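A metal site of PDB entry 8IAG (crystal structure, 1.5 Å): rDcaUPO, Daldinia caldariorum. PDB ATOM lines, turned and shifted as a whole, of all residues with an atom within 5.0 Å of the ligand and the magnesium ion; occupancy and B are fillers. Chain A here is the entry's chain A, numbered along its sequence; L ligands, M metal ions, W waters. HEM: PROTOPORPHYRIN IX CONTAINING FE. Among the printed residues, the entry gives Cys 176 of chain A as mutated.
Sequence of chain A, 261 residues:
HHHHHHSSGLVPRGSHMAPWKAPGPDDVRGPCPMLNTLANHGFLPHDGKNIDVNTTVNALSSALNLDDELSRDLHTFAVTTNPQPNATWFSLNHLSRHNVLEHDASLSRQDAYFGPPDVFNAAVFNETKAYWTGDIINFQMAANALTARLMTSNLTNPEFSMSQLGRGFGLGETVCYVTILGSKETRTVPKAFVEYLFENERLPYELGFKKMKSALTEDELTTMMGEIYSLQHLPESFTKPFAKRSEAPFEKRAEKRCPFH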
ATOM      1  N   PRO A  31     -22.132  21.912  17.193  1.00  0.00           N
ATOM      2  CA  PRO A  31     -21.421  20.980  16.302  1.00  0.00           C
ATOM      3  C   PRO A  31     -22.342  20.423  15.213  1.00  0.00           C
ATOM      4  O   PRO A  31     -21.862  19.661  14.377  1.00  0.00           O
ATOM      5  CB  PRO A  31     -20.980  19.867  17.241  1.00  0.00           C
ATOM      6  CG  PRO A  31     -22.183  19.789  18.206  1.00  0.00           C
ATOM      7  CD  PRO A  31     -22.619  21.225  18.411  1.00  0.00           C
ATOM      8  N   CYS A  32     -23.610  20.789  15.240  1.00  0.00           N
ATOM      9  CA  CYS A  32     -24.562  20.265  14.256  1.00  0.00           C
ATOM     10  C   CYS A  32     -24.706  21.235  13.109  1.00  0.00           C
ATOM     11  O   CYS A  32     -25.202  22.355  13.305  1.00  0.00           O
ATOM     12  CB  CYS A  32     -25.929  20.012  14.888  1.00  0.00           C
ATOM     13  SG  CYS A  32     -27.098  19.407  13.615  1.00  0.00           S
ATOM     14  N   PRO A  33     -24.304  20.825  11.906  1.00  0.00           N
ATOM     15  CA  PRO A  33     -24.429  21.783  10.797  1.00  0.00           C
ATOM     16  C   PRO A  33     -25.886  22.196  10.533  1.00  0.00           C
ATOM     17  O   PRO A  33     -26.140  23.314  10.094  1.00  0.00           O
ATOM     18  CB  PRO A  33     -23.853  21.030   9.602  1.00  0.00           C
ATOM     19  CG  PRO A  33     -24.001  19.552   9.971  1.00  0.00           C
ATOM     20  CD  PRO A  33     -23.804  19.505  11.478  1.00  0.00           C
ATOM     21  N   MET A  34     -26.835  21.283  10.774  1.00  0.00           N
ATOM     22  CA  MET A  34     -28.211  21.624  10.464  1.00  0.00           C
ATOM     23  C   MET A  34     -28.822  22.555  11.503  1.00  0.00           C
ATOM     24  O   MET A  34     -29.444  23.539  11.136  1.00  0.00           O
ATOM     25  CB  MET A  34     -29.063  20.363  10.316  1.00  0.00           C
ATOM     26  CG  MET A  34     -30.533  20.696   9.953  1.00  0.00           C
ATOM     27  SD  MET A  34     -30.724  21.720   8.466  1.00  0.00           S
ATOM     28  CE  MET A  34     -30.566  20.444   7.201  1.00  0.00           C
ATOM     29  N   LEU A  35     -28.618  22.288  12.791  1.00  0.00           N
ATOM     30  CA  LEU A  35     -29.180  23.228  13.769  1.00  0.00           C
ATOM     31  C   LEU A  35     -28.551  24.602  13.615  1.00  0.00           C
ATOM     32  O   LEU A  35     -29.237  25.622  13.765  1.00  0.00           O
ATOM     33  CB  LEU A  35     -29.036  22.727  15.205  1.00  0.00           C
ATOM     34  CG  LEU A  35     -29.756  21.416  15.518  1.00  0.00           C
ATOM     35  CD1 LEU A  35     -29.692  21.196  17.020  1.00  0.00           C
ATOM     36  CD2 LEU A  35     -31.210  21.416  15.009  1.00  0.00           C
ATOM     37  N   THR A  56     -38.421  23.445  18.865  1.00  0.00           N
ATOM     38  CA  THR A  56     -37.750  22.370  18.121  1.00  0.00           C
ATOM     39  C   THR A  56     -38.687  21.633  17.179  1.00  0.00           C
ATOM     40  O   THR A  56     -38.393  21.472  16.002  1.00  0.00           O
ATOM     41  CB  THR A  56     -37.144  21.350  19.080  1.00  0.00           C
ATOM     42  OG1 THR A  56     -36.188  22.030  19.899  1.00  0.00           O
ATOM     43  CG2 THR A  56     -36.461  20.215  18.318  1.00  0.00           C
ATOM     44  N   LEU A  60     -38.282  22.000  13.055  1.00  0.00           N
ATOM     45  CA  LEU A  60     -37.886  20.871  12.221  1.00  0.00           C
ATOM     46  C   LEU A  60     -39.021  20.505  11.266  1.00  0.00           C
ATOM     47  O   LEU A  60     -38.779  20.013  10.161  1.00  0.00           O
ATOM     48  CB  LEU A  60     -37.489  19.672  13.094  1.00  0.00           C
ATOM     49  CG  LEU A  60     -36.208  19.935  13.890  1.00  0.00           C
ATOM     50  CD1 LEU A  60     -35.873  18.740  14.802  1.00  0.00           C
ATOM     51  CD2 LEU A  60     -35.055  20.191  12.945  1.00  0.00           C
ATOM     52  N   LEU A  64     -37.944  21.394   7.457  1.00  0.00           N
ATOM     53  CA  LEU A  64     -37.457  20.119   6.916  1.00  0.00           C
ATOM     54  C   LEU A  64     -38.508  19.035   6.790  1.00  0.00           C
ATOM     55  O   LEU A  64     -38.240  17.977   6.224  1.00  0.00           O
ATOM     56  CB  LEU A  64     -36.302  19.599   7.790  1.00  0.00           C
ATOM     57  CG  LEU A  64     -35.124  20.561   7.969  1.00  0.00           C
ATOM     58  CD1 LEU A  64     -34.123  20.000   8.991  1.00  0.00           C
ATOM     59  CD2 LEU A  64     -34.427  20.826   6.633  1.00  0.00           C
ATOM     60  N   LEU A  66     -39.732  17.074   9.183  1.00  0.00           N
ATOM     61  CA  LEU A  66     -39.554  15.883  10.011  1.00  0.00           C
ATOM     62  C   LEU A  66     -40.824  15.586  10.802  1.00  0.00           C
ATOM     63  O   LEU A  66     -41.527  16.517  11.223  1.00  0.00           O
ATOM     64  CB  LEU A  66     -38.387  16.076  10.978  1.00  0.00           C
ATOM     65  CG  LEU A  66     -37.056  16.472  10.364  1.00  0.00           C
ATOM     66  CD1 LEU A  66     -35.981  16.294  11.437  1.00  0.00           C
ATOM     67  CD2 LEU A  66     -36.773  15.652   9.101  1.00  0.00           C
ATOM     68  N   LEU A  74     -35.340  13.897  19.288  1.00  0.00           N
ATOM     69  CA  LEU A  74     -34.088  14.634  19.151  1.00  0.00           C
ATOM     70  C   LEU A  74     -33.957  15.715  20.238  1.00  0.00           C
ATOM     71  O   LEU A  74     -32.877  15.907  20.806  1.00  0.00           O
ATOM     72  CB  LEU A  74     -33.971  15.278  17.777  1.00  0.00           C
ATOM     73  CG  LEU A  74     -33.776  14.255  16.669  1.00  0.00           C
ATOM     74  CD1 LEU A  74     -33.872  14.947  15.299  1.00  0.00           C
ATOM     75  CD2 LEU A  74     -32.425  13.584  16.831  1.00  0.00           C
ATOM     76  N   HIS A  75     -35.067  16.397  20.540  1.00  0.00           N
ATOM     77  CA  HIS A  75     -35.053  17.399  21.598  1.00  0.00           C
ATOM     78  C   HIS A  75     -34.694  16.762  22.943  1.00  0.00           C
ATOM     79  O   HIS A  75     -33.954  17.346  23.734  1.00  0.00           O
ATOM     80  CB  HIS A  75     -36.414  18.099  21.703  1.00  0.00           C
ATOM     81  CG  HIS A  75     -36.397  19.262  22.646  1.00  0.00           C
ATOM     82  ND1 HIS A  75     -35.954  20.514  22.289  1.00  0.00           N
ATOM     83  CD2 HIS A  75     -36.762  19.345  23.945  1.00  0.00           C
ATOM     84  CE1 HIS A  75     -36.034  21.322  23.333  1.00  0.00           C
ATOM     85  NE2 HIS A  75     -36.523  20.634  24.355  1.00  0.00           N
ATOM     86  N   ALA A  78     -31.132  16.371  23.110  1.00  0.00           N
ATOM     87  CA  ALA A  78     -30.470  17.666  23.203  1.00  0.00           C
ATOM     88  C   ALA A  78     -30.439  18.193  24.629  1.00  0.00           C
ATOM     89  O   ALA A  78     -29.427  18.730  25.074  1.00  0.00           O
ATOM     90  CB  ALA A  78     -31.151  18.689  22.289  1.00  0.00           C
ATOM     91  N   PHE A  90     -32.527  23.741  25.624  1.00  0.00           N
ATOM     92  CA  PHE A  90     -31.088  23.719  25.447  1.00  0.00           C
ATOM     93  C   PHE A  90     -30.638  24.877  24.578  1.00  0.00           C
ATOM     94  O   PHE A  90     -31.462  25.555  23.948  1.00  0.00           O
ATOM     95  CB  PHE A  90     -30.619  22.388  24.806  1.00  0.00           C
ATOM     96  CG  PHE A  90     -30.997  22.248  23.341  1.00  0.00           C
ATOM     97  CD1 PHE A  90     -32.302  21.914  22.981  1.00  0.00           C
ATOM     98  CD2 PHE A  90     -30.051  22.451  22.333  1.00  0.00           C
ATOM     99  CE1 PHE A  90     -32.653  21.794  21.635  1.00  0.00           C
ATOM    100  CE2 PHE A  90     -30.403  22.322  20.982  1.00  0.00           C
ATOM    101  CZ  PHE A  90     -31.700  21.999  20.644  1.00  0.00           C
ATOM    102  N   LEU A  95     -24.507  21.635  23.133  1.00  0.00           N
ATOM    103  CA  LEU A  95     -24.324  20.429  22.317  1.00  0.00           C
ATOM    104  C   LEU A  95     -22.868  20.083  22.036  1.00  0.00           C
ATOM    105  O   LEU A  95     -22.566  18.948  21.634  1.00  0.00           O
ATOM    106  CB  LEU A  95     -25.040  20.575  20.978  1.00  0.00           C
ATOM    107  CG  LEU A  95     -26.549  20.755  21.035  1.00  0.00           C
ATOM    108  CD1 LEU A  95     -27.065  21.000  19.625  1.00  0.00           C
ATOM    109  CD2 LEU A  95     -27.207  19.514  21.617  1.00  0.00           C
ATOM    110  N   LEU A 101     -23.188  14.176  23.451  1.00  0.00           N
ATOM    111  CA  LEU A 101     -23.728  13.850  22.121  1.00  0.00           C
ATOM    112  C   LEU A 101     -22.671  14.033  21.037  1.00  0.00           C
ATOM    113  O   LEU A 101     -22.692  13.346  19.997  1.00  0.00           O
ATOM    114  CB  LEU A 101     -24.945  14.729  21.790  1.00  0.00           C
ATOM    115  CG  LEU A 101     -26.122  14.610  22.742  1.00  0.00           C
ATOM    116  CD1 LEU A 101     -27.269  15.456  22.201  1.00  0.00           C
ATOM    117  CD2 LEU A 101     -26.562  13.154  22.912  1.00  0.00           C
ATOM    118  N   GLU A 102     -21.769  14.984  21.248  1.00  0.00           N
ATOM    119  CA  GLU A 102     -20.630  15.180  20.348  1.00  0.00           C
ATOM    120  C   GLU A 102     -19.665  14.002  20.449  1.00  0.00           C
ATOM    121  O   GLU A 102     -19.424  13.480  21.535  1.00  0.00           O
ATOM    122  CB  GLU A 102     -19.941  16.503  20.686  1.00  0.00           C
ATOM    123  CG  GLU A 102     -18.892  16.961  19.669  1.00  0.00           C
ATOM    124  CD  GLU A 102     -17.595  16.168  19.728  1.00  0.00           C
ATOM    125  OE1 GLU A 102     -17.148  15.798  20.847  1.00  0.00           O
ATOM    126  OE2 GLU A 102     -17.020  15.908  18.642  1.00  0.00           O
ATOM    127  N   HIS A 103     -19.108  13.600  19.311  1.00  0.00           N
ATOM    128  CA  HIS A 103     -18.210  12.430  19.269  1.00  0.00           C
ATOM    129  C   HIS A 103     -17.094  12.619  18.247  1.00  0.00           C
ATOM    130  O   HIS A 103     -17.151  13.454  17.337  1.00  0.00           O
ATOM    131  CB  HIS A 103     -18.997  11.154  18.943  1.00  0.00           C
ATOM    132  CG  HIS A 103     -19.851  11.291  17.716  1.00  0.00           C
ATOM    133  ND1 HIS A 103     -19.329  11.221  16.436  1.00  0.00           N
ATOM    134  CD2 HIS A 103     -21.168  11.582  17.583  1.00  0.00           C
ATOM    135  CE1 HIS A 103     -20.298  11.455  15.570  1.00  0.00           C
ATOM    136  NE2 HIS A 103     -21.419  11.666  16.234  1.00  0.00           N
ATOM    137  N   ASP A 104     -16.073  11.783  18.393  1.00  0.00           N
ATOM    138  CA  ASP A 104     -14.986  11.712  17.419  1.00  0.00           C
ATOM    139  C   ASP A 104     -15.457  11.229  16.052  1.00  0.00           C
ATOM    140  O   ASP A 104     -16.590  10.764  15.892  1.00  0.00           O
ATOM    141  CB  ASP A 104     -13.894  10.765  17.919  1.00  0.00           C
ATOM    142  CG  ASP A 104     -13.200  11.255  19.171  1.00  0.00           C
ATOM    143  OD1 ASP A 104     -13.174  12.492  19.419  1.00  0.00           O
ATOM    144  OD2 ASP A 104     -12.667  10.398  19.902  1.00  0.00           O
ATOM    145  N   SER A 106     -16.148  12.851  13.361  1.00  0.00           N
ATOM    146  CA  SER A 106     -17.104  13.692  12.649  1.00  0.00           C
ATOM    147  C   SER A 106     -16.642  13.927  11.215  1.00  0.00           C
ATOM    148  O   SER A 106     -15.441  13.848  10.888  1.00  0.00           O
ATOM    149  CB  SER A 106     -17.263  15.035  13.370  1.00  0.00           C
ATOM    150  OG  SER A 106     -17.850  14.825  14.659  1.00  0.00           O
ATOM    151  N   LEU A 107     -17.616  14.230  10.350  1.00  0.00           N
ATOM    152  CA  LEU A 107     -17.362  14.410   8.936  1.00  0.00           C
ATOM    153  C   LEU A 107     -16.742  15.766   8.598  1.00  0.00           C
ATOM    154  O   LEU A 107     -16.104  15.921   7.553  1.00  0.00           O
ATOM    155  CB  LEU A 107     -18.677  14.253   8.163  1.00  0.00           C
ATOM    156  CG  LEU A 107     -19.454  12.954   8.423  1.00  0.00           C
ATOM    157  CD1 LEU A 107     -20.736  12.945   7.613  1.00  0.00           C
ATOM    158  CD2 LEU A 107     -18.611  11.725   8.096  1.00  0.00           C
ATOM    159  N   SER A 108     -16.943  16.761   9.458  1.00  0.00           N
ATOM    160  CA  SER A 108     -16.575  18.131   9.127  1.00  0.00           C
ATOM    161  C   SER A 108     -15.952  18.887  10.271  1.00  0.00           C
ATOM    162  O   SER A 108     -15.665  20.086  10.139  1.00  0.00           O
ATOM    163  CB  SER A 108     -17.800  18.929   8.637  1.00  0.00           C
ATOM    164  OG  SER A 108     -18.756  19.138   9.678  1.00  0.00           O
ATOM    165  N   ARG A 109     -15.780  18.227  11.422  1.00  0.00           N
ATOM    166  CA  ARG A 109     -15.220  18.838  12.641  1.00  0.00           C
ATOM    167  C   ARG A 109     -13.979  18.079  13.063  1.00  0.00           C
ATOM    168  O   ARG A 109     -13.896  16.865  12.821  1.00  0.00           O
ATOM    169  CB  ARG A 109     -16.229  18.800  13.790  1.00  0.00           C
ATOM    170  CG  ARG A 109     -17.172  19.991  13.900  1.00  0.00           C
ATOM    171  CD  ARG A 109     -18.011  20.227  12.661  1.00  0.00           C
ATOM    172  NE  ARG A 109     -18.843  21.411  12.907  1.00  0.00           N
ATOM    173  CZ  ARG A 109     -19.575  22.026  11.997  1.00  0.00           C
ATOM    174  NH1 ARG A 109     -19.617  21.569  10.751  1.00  0.00           N
ATOM    175  NH2 ARG A 109     -20.262  23.122  12.335  1.00  0.00           N
ATOM    176  N   GLN A 110     -13.042  18.764  13.719  1.00  0.00           N
ATOM    177  CA  GLN A 110     -11.927  18.089  14.369  1.00  0.00           C
ATOM    178  C   GLN A 110     -12.390  17.226  15.545  1.00  0.00           C
ATOM    179  O   GLN A 110     -13.381  17.561  16.220  1.00  0.00           O
ATOM    180  CB  GLN A 110     -10.909  19.100  14.877  1.00  0.00           C
ATOM    181  CG  GLN A 110     -10.238  19.860  13.750  1.00  0.00           C
ATOM    182  CD  GLN A 110      -9.020  20.612  14.239  1.00  0.00           C
ATOM    183  OE1 GLN A 110      -7.898  20.078  14.218  1.00  0.00           O
ATOM    184  NE2 GLN A 110      -9.224  21.832  14.702  1.00  0.00           N
ATOM    185  N   PRO A 117     -14.258  20.924  18.808  1.00  0.00           N
ATOM    186  CA  PRO A 117     -15.031  20.022  17.947  1.00  0.00           C
ATOM    187  C   PRO A 117     -16.360  20.625  17.524  1.00  0.00           C
ATOM    188  O   PRO A 117     -17.258  19.891  17.122  1.00  0.00           O
ATOM    189  CB  PRO A 117     -15.238  18.790  18.832  1.00  0.00           C
ATOM    190  CG  PRO A 117     -15.364  19.403  20.209  1.00  0.00           C
ATOM    191  CD  PRO A 117     -14.340  20.521  20.223  1.00  0.00           C
ATOM    192  N   GLU A 173     -26.549  10.536  11.888  1.00  0.00           N
ATOM    193  CA  GLU A 173     -26.110  11.785  11.261  1.00  0.00           C
ATOM    194  C   GLU A 173     -25.928  11.585   9.751  1.00  0.00           C
ATOM    195  O   GLU A 173     -26.314  12.450   8.948  1.00  0.00           O
ATOM    196  CB  GLU A 173     -24.825  12.288  11.927  1.00  0.00           C
ATOM    197  CG  GLU A 173     -25.041  12.743  13.385  1.00  0.00           C
ATOM    198  CD  GLU A 173     -23.837  12.463  14.281  1.00  0.00           C
ATOM    199  OE1 GLU A 173     -22.752  12.159  13.758  1.00  0.00           O
ATOM    200  OE2 GLU A 173     -24.012  12.521  15.520  1.00  0.00           O
ATOM    201  N   CYS A 176     -29.203  11.296   8.062  1.00  0.00           N
ATOM    202  CA  CYS A 176     -29.852  12.595   8.033  1.00  0.00           C
ATOM    203  C   CYS A 176     -29.377  13.481   6.875  1.00  0.00           C
ATOM    204  O   CYS A 176     -30.202  14.057   6.161  1.00  0.00           O
ATOM    205  CB  CYS A 176     -29.666  13.318   9.364  1.00  0.00           C
ATOM    206  SG  CYS A 176     -30.797  12.741  10.670  1.00  0.00           S
ATOM    207  N   TYR A 177     -28.067  13.619   6.640  1.00  0.00           N
ATOM    208  CA  TYR A 177     -27.700  14.530   5.551  1.00  0.00           C
ATOM    209  C   TYR A 177     -28.120  13.995   4.187  1.00  0.00           C
ATOM    210  O   TYR A 177     -28.521  14.785   3.335  1.00  0.00           O
ATOM    211  CB  TYR A 177     -26.190  14.878   5.587  1.00  0.00           C
ATOM    212  CG  TYR A 177     -25.184  13.866   5.069  1.00  0.00           C
ATOM    213  CD1 TYR A 177     -25.012  13.650   3.704  1.00  0.00           C
ATOM    214  CD2 TYR A 177     -24.331  13.195   5.958  1.00  0.00           C
ATOM    215  CE1 TYR A 177     -24.050  12.730   3.233  1.00  0.00           C
ATOM    216  CE2 TYR A 177     -23.381  12.281   5.498  1.00  0.00           C
ATOM    217  CZ  TYR A 177     -23.235  12.052   4.140  1.00  0.00           C
ATOM    218  OH  TYR A 177     -22.271  11.166   3.689  1.00  0.00           O
ATOM    219  N   ILE A 180     -32.537  13.914   4.486  1.00  0.00           N
ATOM    220  CA  ILE A 180     -33.254  15.136   4.811  1.00  0.00           C
ATOM    221  C   ILE A 180     -32.945  16.236   3.782  1.00  0.00           C
ATOM    222  O   ILE A 180     -33.809  17.055   3.470  1.00  0.00           O
ATOM    223  CB  ILE A 180     -32.955  15.568   6.265  1.00  0.00           C
ATOM    224  CG1 ILE A 180     -33.513  14.519   7.237  1.00  0.00           C
ATOM    225  CG2 ILE A 180     -33.557  16.947   6.566  1.00  0.00           C
ATOM    226  CD1 ILE A 180     -33.181  14.759   8.717  1.00  0.00           C
ATOM    227  N   LEU A 197     -24.649  22.952   2.452  1.00  0.00           N
ATOM    228  CA  LEU A 197     -25.099  22.998   3.843  1.00  0.00           C
ATOM    229  C   LEU A 197     -23.902  23.072   4.790  1.00  0.00           C
ATOM    230  O   LEU A 197     -23.840  23.934   5.666  1.00  0.00           O
ATOM    231  CB  LEU A 197     -25.968  21.778   4.197  1.00  0.00           C
ATOM    232  CG  LEU A 197     -26.450  21.848   5.650  1.00  0.00           C
ATOM    233  CD1 LEU A 197     -27.744  22.658   5.758  1.00  0.00           C
ATOM    234  CD2 LEU A 197     -26.576  20.469   6.301  1.00  0.00           C
ATOM    235  N   PHE A 198     -22.934  22.180   4.605  1.00  0.00           N
ATOM    236  CA  PHE A 198     -21.799  22.128   5.517  1.00  0.00           C
ATOM    237  C   PHE A 198     -20.925  23.383   5.416  1.00  0.00           C
ATOM    238  O   PHE A 198     -20.512  23.951   6.432  1.00  0.00           O
ATOM    239  CB  PHE A 198     -20.923  20.898   5.226  1.00  0.00           C
ATOM    240  CG  PHE A 198     -21.393  19.618   5.908  1.00  0.00           C
ATOM    241  CD1 PHE A 198     -22.282  18.761   5.282  1.00  0.00           C
ATOM    242  CD2 PHE A 198     -20.870  19.255   7.145  1.00  0.00           C
ATOM    243  CE1 PHE A 198     -22.661  17.565   5.890  1.00  0.00           C
ATOM    244  CE2 PHE A 198     -21.240  18.057   7.756  1.00  0.00           C
ATOM    245  CZ  PHE A 198     -22.146  17.212   7.130  1.00  0.00           C
HETATM  246  CHA HEM L   1     -24.028  16.401  14.029  1.00  0.00           C
HETATM  247  CHB HEM L   1     -27.373  17.241  17.417  1.00  0.00           C
HETATM  248  CHC HEM L   1     -30.790  17.747  13.974  1.00  0.00           C
HETATM  249  CHD HEM L   1     -27.505  16.602  10.596  1.00  0.00           C
HETATM  250  C1A HEM L   1     -24.626  16.649  15.233  1.00  0.00           C
HETATM  251  C2A HEM L   1     -23.943  16.691  16.495  1.00  0.00           C
HETATM  252  C3A HEM L   1     -24.878  16.930  17.441  1.00  0.00           C
HETATM  253  C4A HEM L   1     -26.166  17.028  16.786  1.00  0.00           C
HETATM  254  CMA HEM L   1     -24.628  17.037  18.959  1.00  0.00           C
HETATM  255  CAA HEM L   1     -22.415  16.520  16.657  1.00  0.00           C
HETATM  256  CBA HEM L   1     -22.024  15.050  16.514  1.00  0.00           C
HETATM  257  CGA HEM L   1     -20.585  15.030  16.058  1.00  0.00           C
HETATM  258  O1A HEM L   1     -20.381  15.099  14.818  1.00  0.00           O
HETATM  259  O2A HEM L   1     -19.633  14.976  16.898  1.00  0.00           O
HETATM  260  C1B HEM L   1     -28.574  17.407  16.773  1.00  0.00           C
HETATM  261  C2B HEM L   1     -29.827  17.649  17.439  1.00  0.00           C
HETATM  262  C3B HEM L   1     -30.774  17.799  16.497  1.00  0.00           C
HETATM  263  C4B HEM L   1     -30.155  17.673  15.200  1.00  0.00           C
HETATM  264  CMB HEM L   1     -29.957  17.690  18.976  1.00  0.00           C
HETATM  265  CAB HEM L   1     -32.274  18.091  16.658  1.00  0.00           C
HETATM  266  CBB HEM L   1     -32.769  18.705  17.745  1.00  0.00           C
HETATM  267  C1C HEM L   1     -30.193  17.472  12.754  1.00  0.00           C
HETATM  268  C2C HEM L   1     -30.851  17.445  11.486  1.00  0.00           C
HETATM  269  C3C HEM L   1     -29.951  17.139  10.537  1.00  0.00           C
HETATM  270  C4C HEM L   1     -28.687  16.945  11.202  1.00  0.00           C
HETATM  271  CMC HEM L   1     -32.348  17.722  11.299  1.00  0.00           C
HETATM  272  CAC HEM L   1     -30.272  17.009   9.028  1.00  0.00           C
HETATM  273  CBC HEM L   1     -29.370  17.096   8.046  1.00  0.00           C
HETATM  274  C1D HEM L   1     -26.313  16.401  11.241  1.00  0.00           C
HETATM  275  C2D HEM L   1     -25.131  15.927  10.562  1.00  0.00           C
HETATM  276  C3D HEM L   1     -24.059  15.852  11.619  1.00  0.00           C
HETATM  277  C4D HEM L   1     -24.691  16.294  12.835  1.00  0.00           C
HETATM  278  CMD HEM L   1     -25.000  15.537   9.083  1.00  0.00           C
HETATM  279  CAD HEM L   1     -22.621  15.387  11.422  1.00  0.00           C
HETATM  280  CBD HEM L   1     -21.652  16.559  11.372  1.00  0.00           C
HETATM  281  CGD HEM L   1     -20.252  16.024  11.181  1.00  0.00           C
HETATM  282  O1D HEM L   1     -19.361  16.857  10.847  1.00  0.00           O
HETATM  283  O2D HEM L   1     -20.022  14.812  11.350  1.00  0.00           O
HETATM  284  NA  HEM L   1     -25.984  16.872  15.435  1.00  0.00           N
HETATM  285  NB  HEM L   1     -28.813  17.431  15.406  1.00  0.00           N
HETATM  286  NC  HEM L   1     -28.843  17.169  12.553  1.00  0.00           N
HETATM  287  ND  HEM L   1     -26.027  16.599  12.582  1.00  0.00           N
HETATM  288 FE   HEM L   1     -27.399  17.075  13.988  1.00  0.00          FE
HETATM  289 MG    MG M   1     -17.545  15.439  16.728  1.00  0.00          MG
HETATM  290  O   HOH W   1     -15.501  15.711  16.237  1.00  0.00           O
HETATM  291  O   HOH W   2     -20.960  12.291  11.925  1.00  0.00           O
HETATM  292  O   HOH W   3     -18.064  17.423  16.274  1.00  0.00           O
HETATM  293  O   HOH W   4     -19.794  17.877  14.227  1.00  0.00           O
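Water W2 lies within hydrogen-bond range of the side-chain carboxylate (OE1) of Glu 173 (2.6 Å) and an oxygen (O2D) of the ligand (2.8 Å). Water W4 bridges O of Pro 31 and O1A of the ligand.
O of Leu 60 lies within hydrogen-bond range of N of Leu 66 (3.2 Å). A ring nitrogen (NE2) of His 103 lies within hydrogen-bond range of the side-chain carboxylate of Glu 173 (2.8 Å). The side-chain hydroxyl (OG) of Ser 108 is in hydrogen-bond range of the guanidinium group (NH1) of Arg 109 (2.8 Å). The side-chain sulfur (SG) of Cys 32 sits close to the backbone NH (N) of Leu 35, 3.4 Å away. The backbone NH of Met 34 lies close to the side-chain sulfur of Cys 32 (3.4 Å).
The magnesium ion is bound by the side-chain carboxylate (OE2) of Glu 102 (2.0 Å), water W3 (2.1 Å), the backbone carbonyl oxygen (O) of His 103 (2.1 Å), water W1 (2.1 Å), an oxygen (O2A) of the ligand (2.1 Å) and the side-chain hydroxyl (OG) of Ser 106 (2.2 Å). The magnesium ion has six donor atoms within binding distance.
N of Ser 108 sits at hydrogen-bond distance from O1D of the ligand (2.8 Å). An oxygen (O1D) of the ligand lies within hydrogen-bond range of the side-chain hydroxyl (OG) of Ser 108 (2.6 Å). SG of Cys 32 binds FE of the ligand (2.4 Å). N of Leu 107 sits at hydrogen-bond distance from O2D of the ligand (2.7 Å). The backbone NH (N) of His 103 lies close to an oxygen (O2A) of the ligand, at 2.8 Å.
Three residues have an atom within 4 Å of the magnesium ion: Glu 102, His 103 and Ser 106.
Pro 31 touches the ligand. CD of Pro 33 touches C4D of the ligand, at 3.6 Å. CB of Met 34 touches C3C of the ligand (3.4 Å). Leu 35 touches the ligand. Leu 64 touches the ligand (CD1 to CMC, 3.7 Å). Leu 66 touches the ligand (CD1 to CMC, 3.9 Å). CB of Leu 74 touches CAB of the ligand, at 3.5 Å. CB of Ala 78 touches CMB of the ligand (3.7 Å). O of Leu 95 touches CMA of the ligand, at 3.9 Å. Leu 101 touches the ligand. N of Arg 109 touches O1D of the ligand (3.9 Å). O of Glu 173 touches CMD of the ligand, 3.4 Å away. O of Cys 176 touches CBC of the ligand, 3.7 Å away. CB of Tyr 177 touches CMD of the ligand (3.8 Å). CD1 of Ile 180 touches CAC of the ligand (3.7 Å). CE2 of Phe 198 touches O1D of the ligand, 3.8 Å away. Hydrophobic or aromatic side chains within 4 Å of the ligand: Pro 31, Pro 33, Met 34, Leu 35, Leu 64, Leu 66, Leu 74, Ala 78, Leu 101, His 103, Leu 107, Tyr 177, Ile 180 and Phe 198. 22 residues have an atom within 4 Å of the ligand: Pro 31, Cys 32, Pro 33, Met 34, Leu 35, Leu 64, Leu 66, Leu 74, Ala 78, Leu 95, Leu 101, Glu 102, His 103, Ser 106, Leu 107, Ser 108, Arg 109, Glu 173, Cys 176, Tyr 177, Ile 180 and Phe 198.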
